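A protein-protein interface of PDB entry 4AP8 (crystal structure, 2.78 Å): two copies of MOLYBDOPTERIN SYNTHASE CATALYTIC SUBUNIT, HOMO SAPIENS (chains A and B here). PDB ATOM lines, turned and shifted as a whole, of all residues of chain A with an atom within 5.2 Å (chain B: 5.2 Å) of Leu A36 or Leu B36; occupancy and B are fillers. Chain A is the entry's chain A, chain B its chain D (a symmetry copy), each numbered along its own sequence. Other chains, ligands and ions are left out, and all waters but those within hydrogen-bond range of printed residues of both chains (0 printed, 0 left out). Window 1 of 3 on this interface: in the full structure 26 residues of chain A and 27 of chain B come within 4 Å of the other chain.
Of the printed residues of chain B, Val A38 touches Ile B34 and Leu B36. Printed residues of chain A within 4 Å of Ser B23: Val A19. Of the printed residues of chain A, Ser B35 touches Leu A36 (3.5 Å) and Phe A37 (3.7 Å). Of chain A, only Ser A35 (3.5 Å), Leu A36 (2.9 Å) and Val A38 (3.9 Å) come within 4 Å of Leu B36. Ala B101 touches none of the printed residues of chain A. The nearest printed residue of chain B that does not touch Phe A37 is Leu B36 (5.0 Å).
The backbone carbonyl oxygen (O) of Val A19 lies within hydrogen-bond range of the side-chain hydroxyl (OG) of Ser A23, at 3.3 Å. N of Phe A37 lies within hydrogen-bond range of O of Ile A100, at 2.9 Å. The backbone carbonyl oxygen (O) of Val B19 is in hydrogen-bond range of the side-chain hydroxyl (OG) of Ser B23 (3.3 Å). The backbone carbonyl oxygen (O) of Phe B37 is in hydrogen-bond range of the backbone NH (N) of Ile B100 (2.9 Å).
The backbone carbonyl oxygen (O) of Ile A34 is in hydrogen-bond range of the backbone NH (N) of Val B38, 2.8 Å away. The backbone NH of Leu B36 lies within hydrogen-bond range of the backbone carbonyl oxygen of Leu A36 (2.9 Å). The backbone NH of Val A38 sits at hydrogen-bond distance from the backbone carbonyl oxygen of Ile B34 (2.8 Å).
Among the printed residues, pairs that only touch across the chains: Val A19 with Ser B23 (3.5 Å), Ser A23 with Val B19 (3.6 Å), Ile A34 with Phe B37 (3.6 Å), Ser A35 with Leu B36 (3.5 Å), Ser A35 with Phe B37 (3.6 Å), Leu A36 with Ser B35 (3.5 Å), Phe A37 with Ile B34 (3.6 Å), Phe A37 with Ser B35 (3.7 Å) and Val A38 with Leu B36 (3.9 Å).
Val A19 touches Ser B23, and with the chains exchanged Ser A23 touches Val B19. Ile A34 touches Phe B37, and with the chains exchanged Phe A37 touches Ile B34. Ser A35 touches Phe B37, and with the chains exchanged Phe A37 touches Ser B35. Val A38 touches Leu B36, but with the chains exchanged Leu A36 does not touch Val B38 (4.1 Å).
Of the 12 printed residues of chain A, 7 touch a printed residue of chain B. Hydrophobic or aromatic side chains of chain A that line the printed part of chain B: Val A19, Leu A36, Phe A37 and Val A38. Of the 12 printed residues of chain B, 7 touch a printed residue of chain A. Hydrophobic or aromatic side chains of chain B that line the printed part of chain A: Val B19, Ile B34, Leu B36, Phe B37 and Val B38. Among the printed residues, 12 pairs touch across the chains. Among the printed residues, no Asp or Glu carboxylate lies within 4 Å of a Lys or Arg side-chain nitrogen of the other chain.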
ATOM      1  N   VAL A  19      -3.768  19.551  17.938  1.00  0.00           N
ATOM      2  CA  VAL A  19      -4.036  18.125  17.919  1.00  0.00           C
ATOM      3  C   VAL A  19      -5.277  17.807  18.791  1.00  0.00           C
ATOM      4  O   VAL A  19      -6.133  17.017  18.431  1.00  0.00           O
ATOM      5  CB  VAL A  19      -2.781  17.342  18.338  1.00  0.00           C
ATOM      6  CG1 VAL A  19      -2.047  18.076  19.464  1.00  0.00           C
ATOM      7  CG2 VAL A  19      -3.211  15.946  18.763  1.00  0.00           C
ATOM      8  N   VAL A  22      -8.540  18.888  16.741  1.00  0.00           N
ATOM      9  CA  VAL A  22      -8.786  17.997  15.597  1.00  0.00           C
ATOM     10  C   VAL A  22      -9.307  16.625  16.051  1.00  0.00           C
ATOM     11  O   VAL A  22     -10.294  16.126  15.524  1.00  0.00           O
ATOM     12  CB  VAL A  22      -7.547  17.849  14.690  1.00  0.00           C
ATOM     13  CG1 VAL A  22      -7.822  16.862  13.569  1.00  0.00           C
ATOM     14  CG2 VAL A  22      -7.194  19.177  14.070  1.00  0.00           C
ATOM     15  N   SER A  23      -8.686  16.032  17.059  1.00  0.00           N
ATOM     16  CA  SER A  23      -9.227  14.791  17.624  1.00  0.00           C
ATOM     17  C   SER A  23     -10.689  14.920  18.008  1.00  0.00           C
ATOM     18  O   SER A  23     -11.451  14.016  17.698  1.00  0.00           O
ATOM     19  CB  SER A  23      -8.447  14.349  18.836  1.00  0.00           C
ATOM     20  OG  SER A  23      -8.555  15.310  19.865  1.00  0.00           O
ATOM     21  N   ILE A  34      -9.212   5.950  17.051  1.00  0.00           N
ATOM     22  CA  ILE A  34      -8.918   7.185  16.356  1.00  0.00           C
ATOM     23  C   ILE A  34      -7.427   7.148  16.080  1.00  0.00           C
ATOM     24  O   ILE A  34      -6.643   6.960  17.020  1.00  0.00           O
ATOM     25  CB  ILE A  34      -9.165   8.398  17.241  1.00  0.00           C
ATOM     26  CG1 ILE A  34     -10.631   8.540  17.602  1.00  0.00           C
ATOM     27  CG2 ILE A  34      -8.721   9.604  16.508  1.00  0.00           C
ATOM     28  CD1 ILE A  34     -10.964   9.740  18.488  1.00  0.00           C
ATOM     29  N   SER A  35      -7.035   7.310  14.824  1.00  0.00           N
ATOM     30  CA  SER A  35      -5.623   7.376  14.486  1.00  0.00           C
ATOM     31  C   SER A  35      -5.317   8.767  14.022  1.00  0.00           C
ATOM     32  O   SER A  35      -6.187   9.426  13.480  1.00  0.00           O
ATOM     33  CB  SER A  35      -5.282   6.377  13.409  1.00  0.00           C
ATOM     34  OG  SER A  35      -5.345   5.051  13.918  1.00  0.00           O
ATOM     35  N   LEU A  36      -4.125   9.272  14.336  1.00  0.00           N
ATOM     36  CA  LEU A  36      -3.762  10.619  13.907  1.00  0.00           C
ATOM     37  C   LEU A  36      -2.380  10.662  13.349  1.00  0.00           C
ATOM     38  O   LEU A  36      -1.502   9.853  13.723  1.00  0.00           O
ATOM     39  CB  LEU A  36      -3.855  11.652  15.030  1.00  0.00           C
ATOM     40  CG  LEU A  36      -5.165  11.792  15.811  1.00  0.00           C
ATOM     41  CD1 LEU A  36      -4.887  11.206  17.167  1.00  0.00           C
ATOM     42  CD2 LEU A  36      -5.669  13.184  16.036  1.00  0.00           C
ATOM     43  N   PHE A  37      -2.187  11.610  12.439  1.00  0.00           N
ATOM     44  CA  PHE A  37      -0.855  11.939  12.022  1.00  0.00           C
ATOM     45  C   PHE A  37      -0.665  13.406  12.151  1.00  0.00           C
ATOM     46  O   PHE A  37      -1.530  14.149  11.724  1.00  0.00           O
ATOM     47  CB  PHE A  37      -0.652  11.597  10.595  1.00  0.00           C
ATOM     48  CG  PHE A  37       0.687  11.952  10.113  1.00  0.00           C
ATOM     49  CD1 PHE A  37       1.746  11.133  10.383  1.00  0.00           C
ATOM     50  CD2 PHE A  37       0.893  13.106   9.422  1.00  0.00           C
ATOM     51  CE1 PHE A  37       3.017  11.462   9.970  1.00  0.00           C
ATOM     52  CE2 PHE A  37       2.143  13.441   8.995  1.00  0.00           C
ATOM     53  CZ  PHE A  37       3.218  12.615   9.273  1.00  0.00           C
ATOM     54  N   VAL A  38       0.474  13.791  12.724  1.00  0.00           N
ATOM     55  CA  VAL A  38       0.858  15.174  12.887  1.00  0.00           C
ATOM     56  C   VAL A  38       2.171  15.408  12.152  1.00  0.00           C
ATOM     57  O   VAL A  38       3.153  14.723  12.410  1.00  0.00           O
ATOM     58  CB  VAL A  38       1.044  15.548  14.379  1.00  0.00           C
ATOM     59  CG1 VAL A  38       1.411  17.036  14.513  1.00  0.00           C
ATOM     60  CG2 VAL A  38      -0.214  15.218  15.197  1.00  0.00           C
ATOM     61  N   ILE A  99      -2.359  18.047  10.368  1.00  0.00           N
ATOM     62  CA  ILE A  99      -2.946  17.081  11.260  1.00  0.00           C
ATOM     63  C   ILE A  99      -4.070  16.342  10.515  1.00  0.00           C
ATOM     64  O   ILE A  99      -4.986  16.975  10.035  1.00  0.00           O
ATOM     65  CB  ILE A  99      -3.573  17.737  12.475  1.00  0.00           C
ATOM     66  CG1 ILE A  99      -2.520  18.426  13.311  1.00  0.00           C
ATOM     67  CG2 ILE A  99      -4.231  16.695  13.370  1.00  0.00           C
ATOM     68  CD1 ILE A  99      -3.120  19.119  14.521  1.00  0.00           C
ATOM     69  N   ILE A 100      -3.967  15.013  10.416  1.00  0.00           N
ATOM     70  CA  ILE A 100      -5.003  14.149   9.870  1.00  0.00           C
ATOM     71  C   ILE A 100      -5.507  13.244  10.994  1.00  0.00           C
ATOM     72  O   ILE A 100      -4.719  12.764  11.806  1.00  0.00           O
ATOM     73  CB  ILE A 100      -4.465  13.232   8.775  1.00  0.00           C
ATOM     74  CG1 ILE A 100      -4.028  14.048   7.570  1.00  0.00           C
ATOM     75  CG2 ILE A 100      -5.547  12.243   8.347  1.00  0.00           C
ATOM     76  CD1 ILE A 100      -3.131  13.309   6.599  1.00  0.00           C
ATOM     77  N   ALA A 101      -6.818  13.045  11.050  1.00  0.00           N
ATOM     78  CA  ALA A 101      -7.447  12.184  12.038  1.00  0.00           C
ATOM     79  C   ALA A 101      -8.569  11.381  11.366  1.00  0.00           C
ATOM     80  O   ALA A 101      -9.325  11.907  10.558  1.00  0.00           O
ATOM     81  CB  ALA A 101      -7.998  13.030  13.153  1.00  0.00           C
ATOM     82  N   VAL A 114      -5.266   6.401   7.814  1.00  0.00           N
ATOM     83  CA  VAL A 114      -4.471   7.578   8.092  1.00  0.00           C
ATOM     84  C   VAL A 114      -3.190   7.501   7.304  1.00  0.00           C
ATOM     85  O   VAL A 114      -2.765   8.495   6.712  1.00  0.00           O
ATOM     86  CB  VAL A 114      -4.170   7.729   9.595  1.00  0.00           C
ATOM     87  CG1 VAL A 114      -3.068   8.698   9.791  1.00  0.00           C
ATOM     88  CG2 VAL A 114      -5.378   8.273  10.322  1.00  0.00           C
ATOM     89  N   VAL B  19      -5.165  13.502  24.932  1.00  0.00           N
ATOM     90  CA  VAL B  19      -4.414  13.353  23.685  1.00  0.00           C
ATOM     91  C   VAL B  19      -3.466  14.549  23.556  1.00  0.00           C
ATOM     92  O   VAL B  19      -2.335  14.425  23.111  1.00  0.00           O
ATOM     93  CB  VAL B  19      -5.351  13.164  22.482  1.00  0.00           C
ATOM     94  CG1 VAL B  19      -6.371  14.304  22.488  1.00  0.00           C
ATOM     95  CG2 VAL B  19      -4.584  13.038  21.173  1.00  0.00           C
ATOM     96  N   VAL B  22      -0.297  13.941  25.881  1.00  0.00           N
ATOM     97  CA  VAL B  22       0.566  12.883  25.366  1.00  0.00           C
ATOM     98  C   VAL B  22       1.339  13.306  24.125  1.00  0.00           C
ATOM     99  O   VAL B  22       2.547  13.102  24.042  1.00  0.00           O
ATOM    100  CB  VAL B  22      -0.188  11.591  25.076  1.00  0.00           C
ATOM    101  CG1 VAL B  22       0.703  10.684  24.277  1.00  0.00           C
ATOM    102  CG2 VAL B  22      -0.625  10.927  26.391  1.00  0.00           C
ATOM    103  N   SER B  23       0.672  13.919  23.162  1.00  0.00           N
ATOM    104  CA  SER B  23       1.406  14.461  22.001  1.00  0.00           C
ATOM    105  C   SER B  23       2.581  15.364  22.435  1.00  0.00           C
ATOM    106  O   SER B  23       3.651  15.259  21.863  1.00  0.00           O
ATOM    107  CB  SER B  23       0.477  15.237  21.099  1.00  0.00           C
ATOM    108  OG  SER B  23      -0.051  16.353  21.789  1.00  0.00           O
ATOM    109  N   ILE B  34       4.713  12.789  13.872  1.00  0.00           N
ATOM    110  CA  ILE B  34       4.219  12.171  15.067  1.00  0.00           C
ATOM    111  C   ILE B  34       2.997  11.396  14.662  1.00  0.00           C
ATOM    112  O   ILE B  34       2.090  11.961  14.040  1.00  0.00           O
ATOM    113  CB  ILE B  34       3.733  13.193  16.072  1.00  0.00           C
ATOM    114  CG1 ILE B  34       4.864  14.071  16.524  1.00  0.00           C
ATOM    115  CG2 ILE B  34       3.131  12.481  17.270  1.00  0.00           C
ATOM    116  CD1 ILE B  34       4.358  15.117  17.482  1.00  0.00           C
ATOM    117  N   SER B  35       2.952  10.128  15.013  1.00  0.00           N
ATOM    118  CA  SER B  35       1.756   9.343  14.762  1.00  0.00           C
ATOM    119  C   SER B  35       1.137   9.034  16.096  1.00  0.00           C
ATOM    120  O   SER B  35       1.842   8.876  17.075  1.00  0.00           O
ATOM    121  CB  SER B  35       2.106   8.070  14.008  1.00  0.00           C
ATOM    122  OG  SER B  35       2.487   8.345  12.673  1.00  0.00           O
ATOM    123  N   LEU B  36      -0.184   8.986  16.156  1.00  0.00           N
ATOM    124  CA  LEU B  36      -0.851   8.642  17.399  1.00  0.00           C
ATOM    125  C   LEU B  36      -1.960   7.638  17.188  1.00  0.00           C
ATOM    126  O   LEU B  36      -2.580   7.581  16.134  1.00  0.00           O
ATOM    127  CB  LEU B  36      -1.445   9.865  18.104  1.00  0.00           C
ATOM    128  CG  LEU B  36      -0.538  11.042  18.417  1.00  0.00           C
ATOM    129  CD1 LEU B  36      -0.871  12.109  17.441  1.00  0.00           C
ATOM    130  CD2 LEU B  36      -0.794  11.669  19.770  1.00  0.00           C
ATOM    131  N   PHE B  37      -2.222   6.876  18.237  1.00  0.00           N
ATOM    132  CA  PHE B  37      -3.398   6.087  18.287  1.00  0.00           C
ATOM    133  C   PHE B  37      -4.098   6.314  19.591  1.00  0.00           C
ATOM    134  O   PHE B  37      -3.463   6.319  20.627  1.00  0.00           O
ATOM    135  CB  PHE B  37      -3.058   4.637  18.230  1.00  0.00           C
ATOM    136  CG  PHE B  37      -4.258   3.775  18.286  1.00  0.00           C
ATOM    137  CD1 PHE B  37      -5.011   3.582  17.166  1.00  0.00           C
ATOM    138  CD2 PHE B  37      -4.652   3.214  19.453  1.00  0.00           C
ATOM    139  CE1 PHE B  37      -6.128   2.793  17.199  1.00  0.00           C
ATOM    140  CE2 PHE B  37      -5.764   2.429  19.507  1.00  0.00           C
ATOM    141  CZ  PHE B  37      -6.508   2.215  18.366  1.00  0.00           C
ATOM    142  N   VAL B  38      -5.411   6.453  19.513  1.00  0.00           N
ATOM    143  CA  VAL B  38      -6.252   6.615  20.669  1.00  0.00           C
ATOM    144  C   VAL B  38      -7.303   5.518  20.659  1.00  0.00           C
ATOM    145  O   VAL B  38      -8.063   5.388  19.695  1.00  0.00           O
ATOM    146  CB  VAL B  38      -7.004   7.979  20.665  1.00  0.00           C
ATOM    147  CG1 VAL B  38      -7.883   8.045  21.907  1.00  0.00           C
ATOM    148  CG2 VAL B  38      -6.031   9.152  20.575  1.00  0.00           C
ATOM    149  N   ILE B  99      -3.676   5.697  24.815  1.00  0.00           N
ATOM    150  CA  ILE B  99      -3.069   6.611  23.870  1.00  0.00           C
ATOM    151  C   ILE B  99      -1.610   6.229  23.662  1.00  0.00           C
ATOM    152  O   ILE B  99      -0.861   6.171  24.613  1.00  0.00           O
ATOM    153  CB  ILE B  99      -3.069   8.042  24.380  1.00  0.00           C
ATOM    154  CG1 ILE B  99      -4.483   8.561  24.551  1.00  0.00           C
ATOM    155  CG2 ILE B  99      -2.406   8.923  23.362  1.00  0.00           C
ATOM    156  CD1 ILE B  99      -4.544   9.997  25.006  1.00  0.00           C
ATOM    157  N   ILE B 100      -1.222   6.003  22.412  1.00  0.00           N
ATOM    158  CA  ILE B 100       0.163   5.802  22.033  1.00  0.00           C
ATOM    159  C   ILE B 100       0.599   6.940  21.115  1.00  0.00           C
ATOM    160  O   ILE B 100      -0.171   7.352  20.247  1.00  0.00           O
ATOM    161  CB  ILE B 100       0.318   4.497  21.243  1.00  0.00           C
ATOM    162  CG1 ILE B 100      -0.020   3.284  22.103  1.00  0.00           C
ATOM    163  CG2 ILE B 100       1.731   4.363  20.717  1.00  0.00           C
ATOM    164  CD1 ILE B 100      -0.478   2.079  21.290  1.00  0.00           C
ATOM    165  N   ALA B 101       1.844   7.392  21.266  1.00  0.00           N
ATOM    166  CA  ALA B 101       2.437   8.387  20.359  1.00  0.00           C
ATOM    167  C   ALA B 101       3.900   8.060  20.116  1.00  0.00           C
ATOM    168  O   ALA B 101       4.598   7.594  21.000  1.00  0.00           O
ATOM    169  CB  ALA B 101       2.313   9.784  20.900  1.00  0.00           C
ATOM    170  N   VAL B 114       3.671   2.983  15.317  1.00  0.00           N
ATOM    171  CA  VAL B 114       2.429   3.090  16.083  1.00  0.00           C
ATOM    172  C   VAL B 114       1.532   1.902  15.811  1.00  0.00           C
ATOM    173  O   VAL B 114       0.979   1.311  16.736  1.00  0.00           O
ATOM    174  CB  VAL B 114       1.663   4.364  15.783  1.00  0.00           C
ATOM    175  CG1 VAL B 114       0.287   4.238  16.344  1.00  0.00           C
ATOM    176  CG2 VAL B 114       2.364   5.532  16.465  1.00  0.00           C
